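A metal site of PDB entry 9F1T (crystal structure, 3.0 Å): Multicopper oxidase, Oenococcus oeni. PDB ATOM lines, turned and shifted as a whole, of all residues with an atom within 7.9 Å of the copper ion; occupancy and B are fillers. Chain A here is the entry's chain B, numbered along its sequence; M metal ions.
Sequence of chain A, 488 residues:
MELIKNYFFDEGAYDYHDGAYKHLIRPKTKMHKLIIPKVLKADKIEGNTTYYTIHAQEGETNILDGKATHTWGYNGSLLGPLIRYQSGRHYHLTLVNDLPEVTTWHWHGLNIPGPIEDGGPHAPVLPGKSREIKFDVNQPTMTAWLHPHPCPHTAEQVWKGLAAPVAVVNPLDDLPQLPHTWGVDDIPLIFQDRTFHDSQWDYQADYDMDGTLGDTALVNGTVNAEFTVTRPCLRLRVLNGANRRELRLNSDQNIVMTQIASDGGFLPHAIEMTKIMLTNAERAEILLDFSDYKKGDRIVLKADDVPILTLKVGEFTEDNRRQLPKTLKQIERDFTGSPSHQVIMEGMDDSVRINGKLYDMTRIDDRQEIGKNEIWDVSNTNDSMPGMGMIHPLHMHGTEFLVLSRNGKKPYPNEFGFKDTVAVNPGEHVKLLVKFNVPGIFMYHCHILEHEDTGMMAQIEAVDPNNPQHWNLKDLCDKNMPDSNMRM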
ATOM      1  N   MET A 209      -0.396 -26.859  12.402  1.00  0.00           N
ATOM      2  CA  MET A 209      -0.563 -26.137  13.655  1.00  0.00           C
ATOM      3  C   MET A 209      -0.204 -27.007  14.857  1.00  0.00           C
ATOM      4  O   MET A 209       0.205 -26.504  15.891  1.00  0.00           O
ATOM      5  CB  MET A 209      -2.002 -25.633  13.780  1.00  0.00           C
ATOM      6  CG  MET A 209      -3.046 -26.723  13.895  1.00  0.00           C
ATOM      7  SD  MET A 209      -4.692 -26.028  14.115  1.00  0.00           S
ATOM      8  CE  MET A 209      -4.302 -24.299  14.420  1.00  0.00           C
ATOM      9  N   ASP A 210      -0.368 -28.331  14.720  1.00  0.00           N
ATOM     10  CA  ASP A 210      -0.061 -29.244  15.811  1.00  0.00           C
ATOM     11  C   ASP A 210       1.435 -29.538  15.842  1.00  0.00           C
ATOM     12  O   ASP A 210       1.878 -30.373  16.630  1.00  0.00           O
ATOM     13  CB  ASP A 210      -0.826 -30.543  15.682  1.00  0.00           C
ATOM     14  CG  ASP A 210      -1.098 -31.296  16.978  1.00  0.00           C
ATOM     15  OD1 ASP A 210      -1.112 -30.643  18.061  1.00  0.00           O
ATOM     16  OD2 ASP A 210      -1.286 -32.545  16.894  1.00  0.00           O
ATOM     17  N   ARG A 244       8.679 -30.277  16.324  1.00  0.00           N
ATOM     18  CA  ARG A 244       7.674 -31.168  16.906  1.00  0.00           C
ATOM     19  C   ARG A 244       8.253 -32.551  17.185  1.00  0.00           C
ATOM     20  O   ARG A 244       7.901 -33.175  18.170  1.00  0.00           O
ATOM     21  CB  ARG A 244       6.471 -31.270  15.959  1.00  0.00           C
ATOM     22  CG  ARG A 244       5.514 -32.425  16.212  1.00  0.00           C
ATOM     23  CD  ARG A 244       4.875 -32.355  17.573  1.00  0.00           C
ATOM     24  NE  ARG A 244       4.187 -33.604  17.910  1.00  0.00           N
ATOM     25  CZ  ARG A 244       4.549 -34.453  18.869  1.00  0.00           C
ATOM     26  NH1 ARG A 244       5.722 -34.328  19.486  1.00  0.00           N
ATOM     27  NH2 ARG A 244       3.751 -35.455  19.199  1.00  0.00           N
ATOM     28  N   MET A 345      -1.912 -27.839  31.263  1.00  0.00           N
ATOM     29  CA  MET A 345      -1.729 -27.849  29.823  1.00  0.00           C
ATOM     30  C   MET A 345      -2.858 -28.664  29.185  1.00  0.00           C
ATOM     31  O   MET A 345      -3.134 -29.775  29.618  1.00  0.00           O
ATOM     32  CB  MET A 345      -0.388 -28.487  29.443  1.00  0.00           C
ATOM     33  CG  MET A 345       0.804 -27.792  30.087  1.00  0.00           C
ATOM     34  SD  MET A 345       2.379 -28.528  29.605  1.00  0.00           S
ATOM     35  CE  MET A 345       2.574 -27.808  27.964  1.00  0.00           C
ATOM     36  N   GLU A 346      -3.488 -28.084  28.149  1.00  0.00           N
ATOM     37  CA  GLU A 346      -4.693 -28.656  27.575  1.00  0.00           C
ATOM     38  C   GLU A 346      -4.746 -28.313  26.089  1.00  0.00           C
ATOM     39  O   GLU A 346      -4.208 -27.301  25.665  1.00  0.00           O
ATOM     40  CB  GLU A 346      -5.923 -28.112  28.301  1.00  0.00           C
ATOM     41  CG  GLU A 346      -5.984 -26.590  28.322  1.00  0.00           C
ATOM     42  CD  GLU A 346      -6.890 -26.016  29.411  1.00  0.00           C
ATOM     43  OE1 GLU A 346      -6.339 -25.328  30.307  1.00  0.00           O
ATOM     44  OE2 GLU A 346      -8.125 -26.247  29.364  1.00  0.00           O
ATOM     45  N   GLY A 347      -5.397 -29.197  25.327  1.00  0.00           N
ATOM     46  CA  GLY A 347      -5.719 -28.940  23.935  1.00  0.00           C
ATOM     47  C   GLY A 347      -4.722 -29.598  22.998  1.00  0.00           C
ATOM     48  O   GLY A 347      -3.765 -30.235  23.418  1.00  0.00           O
ATOM     49  N   MET A 348      -4.969 -29.464  21.707  1.00  0.00           N
ATOM     50  CA  MET A 348      -4.081 -29.964  20.694  1.00  0.00           C
ATOM     51  C   MET A 348      -4.345 -29.067  19.518  1.00  0.00           C
ATOM     52  O   MET A 348      -5.439 -28.503  19.435  1.00  0.00           O
ATOM     53  CB  MET A 348      -4.414 -31.403  20.341  1.00  0.00           C
ATOM     54  CG  MET A 348      -3.702 -32.433  21.169  1.00  0.00           C
ATOM     55  SD  MET A 348      -4.061 -34.076  20.536  1.00  0.00           S
ATOM     56  CE  MET A 348      -4.242 -34.910  22.113  1.00  0.00           C
ATOM     57  N   ASP A 349      -3.382 -28.901  18.623  1.00  0.00           N
ATOM     58  CA  ASP A 349      -3.610 -28.092  17.436  1.00  0.00           C
ATOM     59  C   ASP A 349      -4.032 -26.697  17.843  1.00  0.00           C
ATOM     60  O   ASP A 349      -3.273 -26.003  18.522  1.00  0.00           O
ATOM     61  CB  ASP A 349      -4.618 -28.724  16.491  1.00  0.00           C
ATOM     62  CG  ASP A 349      -4.365 -30.194  16.188  1.00  0.00           C
ATOM     63  OD1 ASP A 349      -4.575 -31.031  17.088  1.00  0.00           O
ATOM     64  OD2 ASP A 349      -3.985 -30.494  15.047  1.00  0.00           O
ATOM     65  N   VAL A 352      -4.837 -25.599  21.889  1.00  0.00           N
ATOM     66  CA  VAL A 352      -3.812 -25.599  22.904  1.00  0.00           C
ATOM     67  C   VAL A 352      -3.843 -24.336  23.762  1.00  0.00           C
ATOM     68  O   VAL A 352      -3.993 -23.231  23.244  1.00  0.00           O
ATOM     69  CB  VAL A 352      -2.464 -25.789  22.196  1.00  0.00           C
ATOM     70  CG1 VAL A 352      -2.352 -27.180  21.601  1.00  0.00           C
ATOM     71  CG2 VAL A 352      -2.244 -24.734  21.129  1.00  0.00           C
ATOM     72  N   ARG A 353      -3.698 -24.508  25.078  1.00  0.00           N
ATOM     73  CA  ARG A 353      -3.827 -23.410  26.007  1.00  0.00           C
ATOM     74  C   ARG A 353      -3.226 -23.743  27.357  1.00  0.00           C
ATOM     75  O   ARG A 353      -3.064 -24.904  27.674  1.00  0.00           O
ATOM     76  CB  ARG A 353      -5.293 -23.151  26.285  1.00  0.00           C
ATOM     77  CG  ARG A 353      -5.977 -22.233  25.298  1.00  0.00           C
ATOM     78  CD  ARG A 353      -7.480 -22.311  25.515  1.00  0.00           C
ATOM     79  NE  ARG A 353      -8.203 -22.289  24.240  1.00  0.00           N
ATOM     80  CZ  ARG A 353      -9.519 -22.352  24.140  1.00  0.00           C
ATOM     81  NH1 ARG A 353     -10.264 -22.422  25.236  1.00  0.00           N
ATOM     82  NH2 ARG A 353     -10.101 -22.328  22.952  1.00  0.00           N
ATOM     83  N   ASN A 380      -1.444 -32.576  32.166  1.00  0.00           N
ATOM     84  CA  ASN A 380      -1.869 -32.654  30.783  1.00  0.00           C
ATOM     85  C   ASN A 380      -3.279 -33.246  30.760  1.00  0.00           C
ATOM     86  O   ASN A 380      -3.483 -34.348  31.232  1.00  0.00           O
ATOM     87  CB  ASN A 380      -0.892 -33.489  29.954  1.00  0.00           C
ATOM     88  CG  ASN A 380      -1.299 -33.615  28.508  1.00  0.00           C
ATOM     89  OD1 ASN A 380      -2.376 -33.169  28.105  1.00  0.00           O
ATOM     90  ND2 ASN A 380      -0.449 -34.238  27.701  1.00  0.00           N
ATOM     91  N   ASN A 382      -5.129 -34.204  28.090  1.00  0.00           N
ATOM     92  CA  ASN A 382      -5.371 -34.693  26.762  1.00  0.00           C
ATOM     93  C   ASN A 382      -5.849 -36.087  27.026  1.00  0.00           C
ATOM     94  O   ASN A 382      -5.613 -36.607  28.106  1.00  0.00           O
ATOM     95  CB  ASN A 382      -4.103 -34.616  25.915  1.00  0.00           C
ATOM     96  CG  ASN A 382      -3.960 -33.325  25.147  1.00  0.00           C
ATOM     97  OD1 ASN A 382      -2.924 -33.099  24.523  1.00  0.00           O
ATOM     98  ND2 ASN A 382      -4.977 -32.470  25.167  1.00  0.00           N
ATOM     99  N   MET A 390      -1.211 -36.422  23.010  1.00  0.00           N
ATOM    100  CA  MET A 390       0.131 -36.049  22.586  1.00  0.00           C
ATOM    101  C   MET A 390       0.953 -35.680  23.809  1.00  0.00           C
ATOM    102  O   MET A 390       0.403 -35.308  24.829  1.00  0.00           O
ATOM    103  CB  MET A 390       0.088 -34.907  21.583  1.00  0.00           C
ATOM    104  CG  MET A 390      -0.038 -33.511  22.148  1.00  0.00           C
ATOM    105  SD  MET A 390      -0.246 -32.451  20.708  1.00  0.00           S
ATOM    106  CE  MET A 390       1.450 -32.403  20.128  1.00  0.00           C
ATOM    107  N   ILE A 391       2.263 -35.816  23.706  1.00  0.00           N
ATOM    108  CA  ILE A 391       3.124 -35.422  24.808  1.00  0.00           C
ATOM    109  C   ILE A 391       3.632 -34.001  24.622  1.00  0.00           C
ATOM    110  O   ILE A 391       4.396 -33.754  23.704  1.00  0.00           O
ATOM    111  CB  ILE A 391       4.302 -36.382  24.996  1.00  0.00           C
ATOM    112  CG1 ILE A 391       3.808 -37.809  25.148  1.00  0.00           C
ATOM    113  CG2 ILE A 391       5.141 -35.977  26.190  1.00  0.00           C
ATOM    114  CD1 ILE A 391       4.740 -38.847  24.548  1.00  0.00           C
ATOM    115  N   HIS A 392       3.186 -33.075  25.489  1.00  0.00           N
ATOM    116  CA  HIS A 392       3.695 -31.707  25.538  1.00  0.00           C
ATOM    117  C   HIS A 392       4.902 -31.644  26.473  1.00  0.00           C
ATOM    118  O   HIS A 392       4.840 -32.171  27.584  1.00  0.00           O
ATOM    119  CB  HIS A 392       2.645 -30.741  26.097  1.00  0.00           C
ATOM    120  CG  HIS A 392       1.330 -30.790  25.393  1.00  0.00           C
ATOM    121  ND1 HIS A 392       0.977 -29.920  24.390  1.00  0.00           N
ATOM    122  CD2 HIS A 392       0.285 -31.595  25.565  1.00  0.00           C
ATOM    123  CE1 HIS A 392      -0.245 -30.205  23.983  1.00  0.00           C
ATOM    124  NE2 HIS A 392      -0.686 -31.225  24.677  1.00  0.00           N
ATOM    125  N   PRO A 393       6.041 -31.045  26.051  1.00  0.00           N
ATOM    126  CA  PRO A 393       7.150 -30.778  26.974  1.00  0.00           C
ATOM    127  C   PRO A 393       7.138 -29.377  27.579  1.00  0.00           C
ATOM    128  O   PRO A 393       7.236 -28.395  26.850  1.00  0.00           O
ATOM    129  CB  PRO A 393       8.333 -31.022  26.017  1.00  0.00           C
ATOM    130  CG  PRO A 393       7.860 -30.481  24.683  1.00  0.00           C
ATOM    131  CD  PRO A 393       6.358 -30.664  24.665  1.00  0.00           C
ATOM    132  N   LEU A 394       6.983 -29.280  28.913  1.00  0.00           N
ATOM    133  CA  LEU A 394       6.990 -27.994  29.587  1.00  0.00           C
ATOM    134  C   LEU A 394       8.448 -27.524  29.709  1.00  0.00           C
ATOM    135  O   LEU A 394       9.297 -28.276  30.193  1.00  0.00           O
ATOM    136  CB  LEU A 394       6.338 -28.006  30.978  1.00  0.00           C
ATOM    137  CG  LEU A 394       6.321 -26.650  31.718  1.00  0.00           C
ATOM    138  CD1 LEU A 394       4.992 -25.928  31.554  1.00  0.00           C
ATOM    139  CD2 LEU A 394       6.678 -26.710  33.203  1.00  0.00           C
ATOM    140  N   HIS A 445       6.236 -22.562  28.903  1.00  0.00           N
ATOM    141  CA  HIS A 445       5.466 -22.893  27.709  1.00  0.00           C
ATOM    142  C   HIS A 445       5.761 -24.293  27.198  1.00  0.00           C
ATOM    143  O   HIS A 445       6.739 -24.931  27.595  1.00  0.00           O
ATOM    144  CB  HIS A 445       5.775 -21.891  26.581  1.00  0.00           C
ATOM    145  CG  HIS A 445       7.189 -21.911  26.104  1.00  0.00           C
ATOM    146  ND1 HIS A 445       7.517 -22.364  24.852  1.00  0.00           N
ATOM    147  CD2 HIS A 445       8.358 -21.548  26.674  1.00  0.00           C
ATOM    148  CE1 HIS A 445       8.822 -22.276  24.663  1.00  0.00           C
ATOM    149  NE2 HIS A 445       9.356 -21.795  25.770  1.00  0.00           N
ATOM    150  N   CYS A 446       4.879 -24.746  26.302  1.00  0.00           N
ATOM    151  CA  CYS A 446       5.078 -25.947  25.522  1.00  0.00           C
ATOM    152  C   CYS A 446       6.108 -25.665  24.435  1.00  0.00           C
ATOM    153  O   CYS A 446       5.957 -24.705  23.693  1.00  0.00           O
ATOM    154  CB  CYS A 446       3.775 -26.402  24.884  1.00  0.00           C
ATOM    155  SG  CYS A 446       3.942 -27.963  23.976  1.00  0.00           S
ATOM    156  N   HIS A 447       7.146 -26.526  24.357  1.00  0.00           N
ATOM    157  CA  HIS A 447       8.284 -26.295  23.488  1.00  0.00           C
ATOM    158  C   HIS A 447       8.120 -26.994  22.144  1.00  0.00           C
ATOM    159  O   HIS A 447       9.075 -27.122  21.385  1.00  0.00           O
ATOM    160  CB  HIS A 447       9.587 -26.722  24.180  1.00  0.00           C
ATOM    161  CG  HIS A 447      10.743 -25.885  23.752  1.00  0.00           C
ATOM    162  ND1 HIS A 447      11.347 -26.031  22.524  1.00  0.00           N
ATOM    163  CD2 HIS A 447      11.376 -24.874  24.355  1.00  0.00           C
ATOM    164  CE1 HIS A 447      12.325 -25.145  22.422  1.00  0.00           C
ATOM    165  NE2 HIS A 447      12.359 -24.427  23.524  1.00  0.00           N
ATOM    166  N   ILE A 448       6.898 -27.468  21.864  1.00  0.00           N
ATOM    167  CA  ILE A 448       6.470 -27.679  20.501  1.00  0.00           C
ATOM    168  C   ILE A 448       6.192 -26.297  19.918  1.00  0.00           C
ATOM    169  O   ILE A 448       5.295 -25.599  20.364  1.00  0.00           O
ATOM    170  CB  ILE A 448       5.255 -28.628  20.426  1.00  0.00           C
ATOM    171  CG1 ILE A 448       5.631 -30.041  20.902  1.00  0.00           C
ATOM    172  CG2 ILE A 448       4.657 -28.659  19.019  1.00  0.00           C
ATOM    173  CD1 ILE A 448       4.457 -30.984  21.054  1.00  0.00           C
ATOM    174  N   LEU A 449       6.995 -25.907  18.914  1.00  0.00           N
ATOM    175  CA  LEU A 449       7.170 -24.502  18.602  1.00  0.00           C
ATOM    176  C   LEU A 449       5.899 -23.921  17.980  1.00  0.00           C
ATOM    177  O   LEU A 449       5.671 -22.723  18.084  1.00  0.00           O
ATOM    178  CB  LEU A 449       8.389 -24.332  17.689  1.00  0.00           C
ATOM    179  CG  LEU A 449       9.732 -24.798  18.253  1.00  0.00           C
ATOM    180  CD1 LEU A 449      10.876 -24.394  17.352  1.00  0.00           C
ATOM    181  CD2 LEU A 449       9.955 -24.274  19.669  1.00  0.00           C
ATOM    182  N   GLU A 450       5.072 -24.761  17.352  1.00  0.00           N
ATOM    183  CA  GLU A 450       3.842 -24.295  16.730  1.00  0.00           C
ATOM    184  C   GLU A 450       2.762 -24.089  17.792  1.00  0.00           C
ATOM    185  O   GLU A 450       1.803 -23.355  17.556  1.00  0.00           O
ATOM    186  CB  GLU A 450       3.365 -25.267  15.654  1.00  0.00           C
ATOM    187  CG  GLU A 450       4.230 -25.244  14.389  1.00  0.00           C
ATOM    188  CD  GLU A 450       5.585 -25.915  14.493  1.00  0.00           C
ATOM    189  OE1 GLU A 450       6.322 -25.853  13.480  1.00  0.00           O
ATOM    190  OE2 GLU A 450       5.909 -26.489  15.558  1.00  0.00           O
ATOM    191  N   HIS A 451       2.903 -24.740  18.944  1.00  0.00           N
ATOM    192  CA  HIS A 451       2.016 -24.501  20.071  1.00  0.00           C
ATOM    193  C   HIS A 451       2.387 -23.182  20.722  1.00  0.00           C
ATOM    194  O   HIS A 451       1.512 -22.382  21.031  1.00  0.00           O
ATOM    195  CB  HIS A 451       2.051 -25.652  21.092  1.00  0.00           C
ATOM    196  CG  HIS A 451       1.475 -26.930  20.587  1.00  0.00           C
ATOM    197  ND1 HIS A 451       1.534 -28.098  21.308  1.00  0.00           N
ATOM    198  CD2 HIS A 451       0.806 -27.225  19.464  1.00  0.00           C
ATOM    199  CE1 HIS A 451       0.940 -29.061  20.627  1.00  0.00           C
ATOM    200  NE2 HIS A 451       0.483 -28.561  19.503  1.00  0.00           N
ATOM    201  N   GLU A 452       3.679 -22.927  20.958  1.00  0.00           N
ATOM    202  CA  GLU A 452       4.084 -21.645  21.521  1.00  0.00           C
ATOM    203  C   GLU A 452       3.602 -20.473  20.672  1.00  0.00           C
ATOM    204  O   GLU A 452       3.107 -19.495  21.199  1.00  0.00           O
ATOM    205  CB  GLU A 452       5.604 -21.585  21.669  1.00  0.00           C
ATOM    206  CG  GLU A 452       6.187 -20.187  21.561  1.00  0.00           C
ATOM    207  CD  GLU A 452       7.689 -20.167  21.767  1.00  0.00           C
ATOM    208  OE1 GLU A 452       8.283 -21.255  21.951  1.00  0.00           O
ATOM    209  OE2 GLU A 452       8.286 -19.068  21.739  1.00  0.00           O
ATOM    210  N   MET A 456       0.576 -21.257  23.538  1.00  0.00           N
ATOM    211  CA  MET A 456       0.693 -22.030  24.755  1.00  0.00           C
ATOM    212  C   MET A 456       1.900 -21.508  25.518  1.00  0.00           C
ATOM    213  O   MET A 456       2.914 -22.191  25.600  1.00  0.00           O
ATOM    214  CB  MET A 456       0.873 -23.518  24.455  1.00  0.00           C
ATOM    215  CG  MET A 456       0.025 -24.465  25.278  1.00  0.00           C
ATOM    216  SD  MET A 456       0.144 -26.158  24.658  1.00  0.00           S
ATOM    217  CE  MET A 456      -0.670 -27.045  25.980  1.00  0.00           C
HETATM  218 CU    CU M   1       1.936 -28.449  23.250  1.00  0.00          CU
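O of His 451 lies within hydrogen-bond range of N of Met 456 (2.9 Å). NE2 of His 451 is in hydrogen-bond range of OD1 of Asp 210, at 3.0 Å. The backbone carbonyl oxygen of Gly 347 sits at hydrogen-bond distance from a ring nitrogen (NE2) of His 392 (3.5 Å). A ring nitrogen (NE2) of His 392 lies within hydrogen-bond range of the side-chain amide oxygen (OD1) of Asn 382 (2.9 Å). The backbone NH (N) of Cys 446 is in hydrogen-bond range of the backbone carbonyl oxygen (O) of Met 456, 3.3 Å away. The side-chain sulfur of Cys 446 lies close to the backbone NH of Ile 448 (3.7 Å).
The copper ion is bound by ND1 of His 451 (2.0 Å), ND1 of His 392 (2.1 Å) and SG of Cys 446 (2.2 Å).
SD of Met 456 touches the copper ion, at 3.2 Å. Of the 26 residues printed, 4 come within 4 Å of the copper ion. Along chain A the residues within 4 Å of the copper ion span positions 392 to 456. The nearest printed residue that does not touch the copper ion is Ile 448 (4.2 Å).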
